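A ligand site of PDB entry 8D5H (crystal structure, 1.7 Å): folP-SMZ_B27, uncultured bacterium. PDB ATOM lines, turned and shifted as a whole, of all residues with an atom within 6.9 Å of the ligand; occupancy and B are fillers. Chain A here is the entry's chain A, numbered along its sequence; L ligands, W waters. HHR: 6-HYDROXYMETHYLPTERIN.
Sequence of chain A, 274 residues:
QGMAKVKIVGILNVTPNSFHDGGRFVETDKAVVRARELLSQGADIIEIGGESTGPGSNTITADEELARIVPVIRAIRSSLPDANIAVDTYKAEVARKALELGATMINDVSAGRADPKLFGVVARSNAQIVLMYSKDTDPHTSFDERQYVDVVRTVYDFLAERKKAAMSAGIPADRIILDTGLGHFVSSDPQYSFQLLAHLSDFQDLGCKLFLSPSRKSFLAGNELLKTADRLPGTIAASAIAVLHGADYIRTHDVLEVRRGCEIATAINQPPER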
ATOM      1  N   ILE A  11      29.474 -31.212 -22.965  1.00  0.00           N
ATOM      2  CA  ILE A  11      29.721 -29.830 -23.383  1.00  0.00           C
ATOM      3  C   ILE A  11      30.564 -29.803 -24.649  1.00  0.00           C
ATOM      4  O   ILE A  11      31.696 -30.334 -24.673  1.00  0.00           O
ATOM      5  CB  ILE A  11      30.433 -29.053 -22.259  1.00  0.00           C
ATOM      6  CG1 ILE A  11      29.579 -29.049 -20.995  1.00  0.00           C
ATOM      7  CG2 ILE A  11      30.747 -27.634 -22.759  1.00  0.00           C
ATOM      8  CD1 ILE A  11      30.394 -28.644 -19.762  1.00  0.00           C
ATOM      9  N   ASN A  13      31.710 -26.530 -26.494  1.00  0.00           N
ATOM     10  CA  ASN A  13      31.759 -25.067 -26.593  1.00  0.00           C
ATOM     11  C   ASN A  13      32.344 -24.648 -27.928  1.00  0.00           C
ATOM     12  O   ASN A  13      33.266 -25.293 -28.438  1.00  0.00           O
ATOM     13  CB  ASN A  13      32.592 -24.461 -25.457  1.00  0.00           C
ATOM     14  CG  ASN A  13      31.881 -24.509 -24.126  1.00  0.00           C
ATOM     15  OD1 ASN A  13      30.647 -24.343 -24.057  1.00  0.00           O
ATOM     16  ND2 ASN A  13      32.635 -24.718 -23.043  1.00  0.00           N
ATOM     17  N   GLU A  47      25.704 -30.439 -26.062  1.00  0.00           N
ATOM     18  CA  GLU A  47      25.319 -29.059 -25.746  1.00  0.00           C
ATOM     19  C   GLU A  47      26.277 -28.060 -26.393  1.00  0.00           C
ATOM     20  O   GLU A  47      27.457 -28.028 -26.077  1.00  0.00           O
ATOM     21  CB  GLU A  47      25.312 -28.865 -24.248  1.00  0.00           C
ATOM     22  CG  GLU A  47      24.986 -27.493 -23.815  1.00  0.00           C
ATOM     23  CD  GLU A  47      24.927 -27.475 -22.305  1.00  0.00           C
ATOM     24  OE1 GLU A  47      25.606 -28.342 -21.710  1.00  0.00           O
ATOM     25  OE2 GLU A  47      24.358 -26.578 -21.721  1.00  0.00           O
ATOM     26  N   THR A  53      29.400 -17.286 -20.486  1.00  0.00           N
ATOM     27  CA  THR A  53      28.713 -16.436 -19.513  1.00  0.00           C
ATOM     28  C   THR A  53      29.359 -16.492 -18.132  1.00  0.00           C
ATOM     29  O   THR A  53      28.746 -16.040 -17.155  1.00  0.00           O
ATOM     30  CB  THR A  53      27.238 -16.823 -19.436  1.00  0.00           C
ATOM     31  OG1 THR A  53      27.121 -18.252 -19.261  1.00  0.00           O
ATOM     32  CG2 THR A  53      26.469 -16.398 -20.714  1.00  0.00           C
ATOM     33  N   GLY A  54      30.597 -17.013 -18.009  1.00  0.00           N
ATOM     34  CA  GLY A  54      31.224 -16.996 -16.694  1.00  0.00           C
ATOM     35  C   GLY A  54      31.789 -15.622 -16.344  1.00  0.00           C
ATOM     36  O   GLY A  54      31.739 -14.661 -17.136  1.00  0.00           O
ATOM     37  N   ASP A  88      23.011 -23.631 -25.712  1.00  0.00           N
ATOM     38  CA  ASP A  88      23.120 -22.656 -24.622  1.00  0.00           C
ATOM     39  C   ASP A  88      22.953 -21.268 -25.187  1.00  0.00           C
ATOM     40  O   ASP A  88      23.867 -20.766 -25.865  1.00  0.00           O
ATOM     41  CB  ASP A  88      24.522 -22.767 -24.019  1.00  0.00           C
ATOM     42  CG  ASP A  88      24.630 -23.846 -23.068  1.00  0.00           C
ATOM     43  OD1 ASP A  88      23.835 -24.764 -23.196  1.00  0.00           O
ATOM     44  OD2 ASP A  88      25.535 -23.792 -22.209  1.00  0.00           O
ATOM     45  N   ASN A 107      19.109 -24.090 -23.240  1.00  0.00           N
ATOM     46  CA  ASN A 107      19.589 -23.841 -21.877  1.00  0.00           C
ATOM     47  C   ASN A 107      19.853 -22.340 -21.733  1.00  0.00           C
ATOM     48  O   ASN A 107      20.758 -21.798 -22.377  1.00  0.00           O
ATOM     49  CB  ASN A 107      20.864 -24.658 -21.642  1.00  0.00           C
ATOM     50  CG  ASN A 107      21.513 -24.322 -20.308  1.00  0.00           C
ATOM     51  OD1 ASN A 107      20.821 -24.064 -19.339  1.00  0.00           O
ATOM     52  ND2 ASN A 107      22.850 -24.257 -20.274  1.00  0.00           N
ATOM     53  N   ASP A 108      19.071 -21.661 -20.877  1.00  0.00           N
ATOM     54  CA  ASP A 108      19.115 -20.203 -20.726  1.00  0.00           C
ATOM     55  C   ASP A 108      19.615 -19.876 -19.323  1.00  0.00           C
ATOM     56  O   ASP A 108      18.850 -19.994 -18.354  1.00  0.00           O
ATOM     57  CB  ASP A 108      17.727 -19.618 -20.959  1.00  0.00           C
ATOM     58  CG  ASP A 108      17.694 -18.102 -20.835  1.00  0.00           C
ATOM     59  OD1 ASP A 108      18.715 -17.487 -20.485  1.00  0.00           O
ATOM     60  OD2 ASP A 108      16.625 -17.522 -21.087  1.00  0.00           O
ATOM     61  N   VAL A 109      20.895 -19.437 -19.232  1.00  0.00           N
ATOM     62  CA  VAL A 109      21.476 -19.105 -17.924  1.00  0.00           C
ATOM     63  C   VAL A 109      20.832 -17.871 -17.286  1.00  0.00           C
ATOM     64  O   VAL A 109      21.133 -17.565 -16.124  1.00  0.00           O
ATOM     65  CB  VAL A 109      23.014 -18.924 -17.963  1.00  0.00           C
ATOM     66  CG1 VAL A 109      23.707 -20.295 -18.400  1.00  0.00           C
ATOM     67  CG2 VAL A 109      23.442 -17.757 -18.933  1.00  0.00           C
ATOM     68  N   VAL A 130      15.848 -25.202 -20.178  1.00  0.00           N
ATOM     69  CA  VAL A 130      16.517 -25.288 -18.864  1.00  0.00           C
ATOM     70  C   VAL A 130      16.545 -23.866 -18.287  1.00  0.00           C
ATOM     71  O   VAL A 130      17.087 -22.955 -18.902  1.00  0.00           O
ATOM     72  CB  VAL A 130      17.947 -25.851 -18.968  1.00  0.00           C
ATOM     73  CG1 VAL A 130      18.547 -26.035 -17.502  1.00  0.00           C
ATOM     74  CG2 VAL A 130      17.955 -27.192 -19.726  1.00  0.00           C
ATOM     75  N   LEU A 131      15.961 -23.681 -17.092  1.00  0.00           N
ATOM     76  CA  LEU A 131      15.964 -22.400 -16.383  1.00  0.00           C
ATOM     77  C   LEU A 131      16.940 -22.538 -15.219  1.00  0.00           C
ATOM     78  O   LEU A 131      16.676 -23.306 -14.299  1.00  0.00           O
ATOM     79  CB  LEU A 131      14.576 -22.049 -15.857  1.00  0.00           C
ATOM     80  CG  LEU A 131      13.449 -22.112 -16.903  1.00  0.00           C
ATOM     81  CD1 LEU A 131      12.055 -21.853 -16.257  1.00  0.00           C
ATOM     82  CD2 LEU A 131      13.759 -21.103 -18.023  1.00  0.00           C
ATOM     83  N   MET A 132      18.045 -21.811 -15.277  1.00  0.00           N
ATOM     84  CA  MET A 132      19.065 -21.770 -14.206  1.00  0.00           C
ATOM     85  C   MET A 132      18.893 -20.569 -13.304  1.00  0.00           C
ATOM     86  O   MET A 132      18.727 -19.444 -13.792  1.00  0.00           O
ATOM     87  CB  MET A 132      20.493 -21.672 -14.752  1.00  0.00           C
ATOM     88  CG  MET A 132      21.564 -22.393 -13.970  1.00  0.00           C
ATOM     89  SD  MET A 132      23.195 -21.770 -14.486  1.00  0.00           S
ATOM     90  CE  MET A 132      23.081 -20.037 -14.375  1.00  0.00           C
ATOM     91  N   ASP A 179      17.490 -25.773 -12.909  1.00  0.00           N
ATOM     92  CA  ASP A 179      18.885 -25.901 -12.450  1.00  0.00           C
ATOM     93  C   ASP A 179      19.098 -24.894 -11.321  1.00  0.00           C
ATOM     94  O   ASP A 179      18.775 -23.712 -11.483  1.00  0.00           O
ATOM     95  CB  ASP A 179      19.780 -25.659 -13.663  1.00  0.00           C
ATOM     96  CG  ASP A 179      21.287 -25.792 -13.408  1.00  0.00           C
ATOM     97  OD1 ASP A 179      21.728 -25.697 -12.239  1.00  0.00           O
ATOM     98  OD2 ASP A 179      22.024 -25.942 -14.427  1.00  0.00           O
ATOM     99  N   GLY A 181      21.730 -23.654 -10.401  1.00  0.00           N
ATOM    100  CA  GLY A 181      23.011 -22.980 -10.516  1.00  0.00           C
ATOM    101  C   GLY A 181      24.029 -23.619  -9.592  1.00  0.00           C
ATOM    102  O   GLY A 181      23.678 -24.251  -8.599  1.00  0.00           O
ATOM    103  N   LEU A 182      25.289 -23.470  -9.964  1.00  0.00           N
ATOM    104  CA  LEU A 182      26.401 -23.845  -9.088  1.00  0.00           C
ATOM    105  C   LEU A 182      27.553 -22.877  -9.359  1.00  0.00           C
ATOM    106  O   LEU A 182      27.586 -22.199 -10.404  1.00  0.00           O
ATOM    107  CB  LEU A 182      26.892 -25.283  -9.336  1.00  0.00           C
ATOM    108  CG  LEU A 182      25.926 -26.439  -8.928  1.00  0.00           C
ATOM    109  CD1 LEU A 182      26.479 -27.817  -9.438  1.00  0.00           C
ATOM    110  CD2 LEU A 182      25.741 -26.492  -7.396  1.00  0.00           C
ATOM    111  N   GLY A 183      28.532 -22.870  -8.445  1.00  0.00           N
ATOM    112  CA  GLY A 183      29.730 -22.038  -8.674  1.00  0.00           C
ATOM    113  C   GLY A 183      29.361 -20.555  -8.620  1.00  0.00           C
ATOM    114  O   GLY A 183      28.461 -20.126  -7.870  1.00  0.00           O
ATOM    115  N   PHE A 185      27.752 -18.589 -10.452  1.00  0.00           N
ATOM    116  CA  PHE A 185      26.352 -18.194 -10.702  1.00  0.00           C
ATOM    117  C   PHE A 185      25.567 -18.065  -9.405  1.00  0.00           C
ATOM    118  O   PHE A 185      24.693 -17.206  -9.258  1.00  0.00           O
ATOM    119  CB  PHE A 185      25.632 -19.204 -11.592  1.00  0.00           C
ATOM    120  CG  PHE A 185      26.236 -19.257 -12.977  1.00  0.00           C
ATOM    121  CD1 PHE A 185      26.007 -18.200 -13.855  1.00  0.00           C
ATOM    122  CD2 PHE A 185      27.063 -20.299 -13.361  1.00  0.00           C
ATOM    123  CE1 PHE A 185      26.584 -18.243 -15.157  1.00  0.00           C
ATOM    124  CE2 PHE A 185      27.642 -20.332 -14.628  1.00  0.00           C
ATOM    125  CZ  PHE A 185      27.393 -19.303 -15.531  1.00  0.00           C
ATOM    126  N   PHE A 211      18.521 -30.347 -13.542  1.00  0.00           N
ATOM    127  CA  PHE A 211      19.720 -30.326 -14.398  1.00  0.00           C
ATOM    128  C   PHE A 211      20.784 -29.632 -13.568  1.00  0.00           C
ATOM    129  O   PHE A 211      20.517 -28.547 -13.026  1.00  0.00           O
ATOM    130  CB  PHE A 211      19.335 -29.550 -15.691  1.00  0.00           C
ATOM    131  CG  PHE A 211      20.434 -29.338 -16.720  1.00  0.00           C
ATOM    132  CD1 PHE A 211      21.520 -28.505 -16.436  1.00  0.00           C
ATOM    133  CD2 PHE A 211      20.280 -29.834 -18.037  1.00  0.00           C
ATOM    134  CE1 PHE A 211      22.484 -28.192 -17.423  1.00  0.00           C
ATOM    135  CE2 PHE A 211      21.208 -29.518 -19.022  1.00  0.00           C
ATOM    136  CZ  PHE A 211      22.338 -28.719 -18.725  1.00  0.00           C
ATOM    137  N   LEU A 212      21.966 -30.229 -13.447  1.00  0.00           N
ATOM    138  CA  LEU A 212      23.025 -29.513 -12.710  1.00  0.00           C
ATOM    139  C   LEU A 212      24.346 -29.694 -13.447  1.00  0.00           C
ATOM    140  O   LEU A 212      24.525 -30.648 -14.225  1.00  0.00           O
ATOM    141  CB  LEU A 212      23.174 -30.092 -11.284  1.00  0.00           C
ATOM    142  CG  LEU A 212      22.273 -29.600 -10.147  1.00  0.00           C
ATOM    143  CD1 LEU A 212      22.906 -29.964  -8.841  1.00  0.00           C
ATOM    144  CD2 LEU A 212      22.153 -28.146 -10.138  1.00  0.00           C
ATOM    145  N   SER A 213      25.289 -28.811 -13.144  1.00  0.00           N
ATOM    146  CA  SER A 213      26.598 -28.842 -13.824  1.00  0.00           C
ATOM    147  C   SER A 213      27.746 -28.548 -12.874  1.00  0.00           C
ATOM    148  O   SER A 213      28.303 -27.448 -12.870  1.00  0.00           O
ATOM    149  CB  SER A 213      26.575 -27.836 -14.977  1.00  0.00           C
ATOM    150  OG  SER A 213      27.728 -27.963 -15.798  1.00  0.00           O
ATOM    151  N   PRO A 214      28.174 -29.529 -12.070  1.00  0.00           N
ATOM    152  CA  PRO A 214      29.365 -29.267 -11.227  1.00  0.00           C
ATOM    153  C   PRO A 214      30.587 -28.927 -12.064  1.00  0.00           C
ATOM    154  O   PRO A 214      31.293 -27.965 -11.770  1.00  0.00           O
ATOM    155  CB  PRO A 214      29.519 -30.567 -10.449  1.00  0.00           C
ATOM    156  CG  PRO A 214      28.063 -31.057 -10.318  1.00  0.00           C
ATOM    157  CD  PRO A 214      27.516 -30.798 -11.719  1.00  0.00           C
ATOM    158  N   SER A 215      30.844 -29.731 -13.107  1.00  0.00           N
ATOM    159  CA  SER A 215      31.806 -29.537 -14.188  1.00  0.00           C
ATOM    160  C   SER A 215      33.070 -28.729 -13.861  1.00  0.00           C
ATOM    161  O   SER A 215      33.328 -27.675 -14.472  1.00  0.00           O
ATOM    162  CB  SER A 215      31.084 -28.907 -15.386  1.00  0.00           C
ATOM    163  OG  SER A 215      30.565 -27.616 -15.128  1.00  0.00           O
ATOM    164  N   LYS A 217      33.910 -26.646 -11.770  1.00  0.00           N
ATOM    165  CA  LYS A 217      33.788 -25.259 -11.346  1.00  0.00           C
ATOM    166  C   LYS A 217      34.677 -24.970 -10.138  1.00  0.00           C
ATOM    167  O   LYS A 217      35.069 -25.887  -9.390  1.00  0.00           O
ATOM    168  CB  LYS A 217      32.319 -24.949 -10.999  1.00  0.00           C
ATOM    169  CG  LYS A 217      31.438 -24.797 -12.254  1.00  0.00           C
ATOM    170  CD  LYS A 217      29.948 -24.617 -11.804  1.00  0.00           C
ATOM    171  CE  LYS A 217      29.075 -24.006 -12.969  1.00  0.00           C
ATOM    172  NZ  LYS A 217      29.011 -24.984 -14.117  1.00  0.00           N
ATOM    173  N   ARG A 251      25.526 -31.945 -16.761  1.00  0.00           N
ATOM    174  CA  ARG A 251      26.278 -31.313 -17.830  1.00  0.00           C
ATOM    175  C   ARG A 251      27.771 -31.378 -17.449  1.00  0.00           C
ATOM    176  O   ARG A 251      28.137 -31.045 -16.319  1.00  0.00           O
ATOM    177  CB  ARG A 251      25.801 -29.879 -17.974  1.00  0.00           C
ATOM    178  CG  ARG A 251      26.663 -28.968 -18.830  1.00  0.00           C
ATOM    179  CD  ARG A 251      26.075 -27.508 -18.770  1.00  0.00           C
ATOM    180  NE  ARG A 251      26.889 -26.624 -19.606  1.00  0.00           N
ATOM    181  CZ  ARG A 251      28.038 -26.079 -19.242  1.00  0.00           C
ATOM    182  NH1 ARG A 251      28.555 -26.282 -18.025  1.00  0.00           N
ATOM    183  NH2 ARG A 251      28.711 -25.334 -20.123  1.00  0.00           N
ATOM    184  N   HIS A 253      32.226 -31.812 -18.967  1.00  0.00           N
ATOM    185  CA  HIS A 253      33.265 -32.036 -19.972  1.00  0.00           C
ATOM    186  C   HIS A 253      33.829 -33.456 -19.915  1.00  0.00           C
ATOM    187  O   HIS A 253      34.488 -33.903 -20.862  1.00  0.00           O
ATOM    188  CB  HIS A 253      34.452 -31.080 -19.765  1.00  0.00           C
ATOM    189  CG  HIS A 253      34.105 -29.770 -19.149  1.00  0.00           C
ATOM    190  ND1 HIS A 253      34.156 -29.557 -17.778  1.00  0.00           N
ATOM    191  CD2 HIS A 253      33.753 -28.578 -19.696  1.00  0.00           C
ATOM    192  CE1 HIS A 253      33.821 -28.302 -17.519  1.00  0.00           C
ATOM    193  NE2 HIS A 253      33.570 -27.690 -18.661  1.00  0.00           N
HETATM  194  C7  HHR L   1      27.477 -22.590 -18.335  1.00  0.00           C
HETATM  195  N8  HHR L   1      26.138 -22.892 -18.557  1.00  0.00           N
HETATM  196  C9  HHR L   1      25.530 -23.505 -17.528  1.00  0.00           C
HETATM  197  N1  HHR L   1      24.210 -23.829 -17.704  1.00  0.00           N
HETATM  198  C2  HHR L   1      23.521 -24.454 -16.753  1.00  0.00           C
HETATM  199  N2  HHR L   1      22.206 -24.738 -16.943  1.00  0.00           N
HETATM  200  C10 HHR L   1      26.211 -23.811 -16.314  1.00  0.00           C
HETATM  201  C4  HHR L   1      25.485 -24.434 -15.311  1.00  0.00           C
HETATM  202  N3  HHR L   1      24.153 -24.776 -15.554  1.00  0.00           N
HETATM  203  O4  HHR L   1      25.978 -24.713 -14.207  1.00  0.00           O
HETATM  204  N5  HHR L   1      27.517 -23.495 -16.140  1.00  0.00           N
HETATM  205  C6  HHR L   1      28.160 -22.886 -17.171  1.00  0.00           C
HETATM  206  C6A HHR L   1      29.536 -22.503 -17.129  1.00  0.00           C
HETATM  207  O6A HHR L   1      30.223 -22.838 -16.007  1.00  0.00           O
HETATM  208  O   HOH W   1      24.567 -26.223 -12.189  1.00  0.00           O
HETATM  209  O   HOH W   2      32.118 -20.367 -15.023  1.00  0.00           O
HETATM  210  O   HOH W   3      31.442 -25.116 -15.767  1.00  0.00           O
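The side-chain carboxylate (OD2) of Asp 179 is in hydrogen-bond range of a nitrogen (N3) of the ligand, 2.7 Å away. A nitrogen (N2) of the ligand lies within hydrogen-bond range of the side-chain amide oxygen (OD1) of Asn 107, 2.8 Å away. NZ of Lys 217 lies within hydrogen-bond range of N5 of the ligand (2.9 Å). A nitrogen (N3) of the ligand lies within hydrogen-bond range of the side-chain sulfur of Met 132 (3.3 Å).
The side-chain carboxylate (OD1) of Asp 179 is in hydrogen-bond range of the backbone NH (N) of Gly 181, 2.7 Å away. N of Asp 179 is in hydrogen-bond range of O of Leu 131, 2.9 Å away. ND2 of Asn 107 lies within hydrogen-bond range of OD1 of Asp 88, at 3.1 Å. NZ of Lys 217 lies within hydrogen-bond range of O of Ser 213, at 2.9 Å. The side-chain hydroxyl (OG) of Ser 215 lies within hydrogen-bond range of the side-chain amino group (NZ) of Lys 217 (3.2 Å). The side-chain carboxylate (OE1) of Glu 47 lies within salt-bridge range of the guanidinium group (NE) of Arg 251, at 3.0 Å. O of Leu 212 is in hydrogen-bond range of N of Arg 251, 3.0 Å away. The backbone carbonyl oxygen (O) of Val 130 lies within hydrogen-bond range of the backbone NH (N) of Asp 108 (3.1 Å).
Asp 88 touches the ligand. Val 109 touches the ligand. Val 130 touches the ligand. CE2 of Phe 185 touches N5 of the ligand, 3.5 Å away. Phe 211 touches the ligand (CE1 to N2, 3.5 Å). Ser 213 touches the ligand (CB to O4, 3.3 Å). Arg 251 touches the ligand. Hydrophobic or aromatic side chains that line the ligand: Val 109, Val 130, Met 132, Phe 185 and Phe 211. The nearest printed residue that does not touch the ligand is Thr 53 (4.4 Å).
Water W3 lies within hydrogen-bond range of O6A of the ligand, OG of Ser 215 and NZ of Lys 217. Water W1 lies within hydrogen-bond range of the backbone NH of Ser 213 (2.9 Å), the side-chain carboxylate of Asp 179 (2.9 Å) and an oxygen (O4) of the ligand (2.9 Å).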
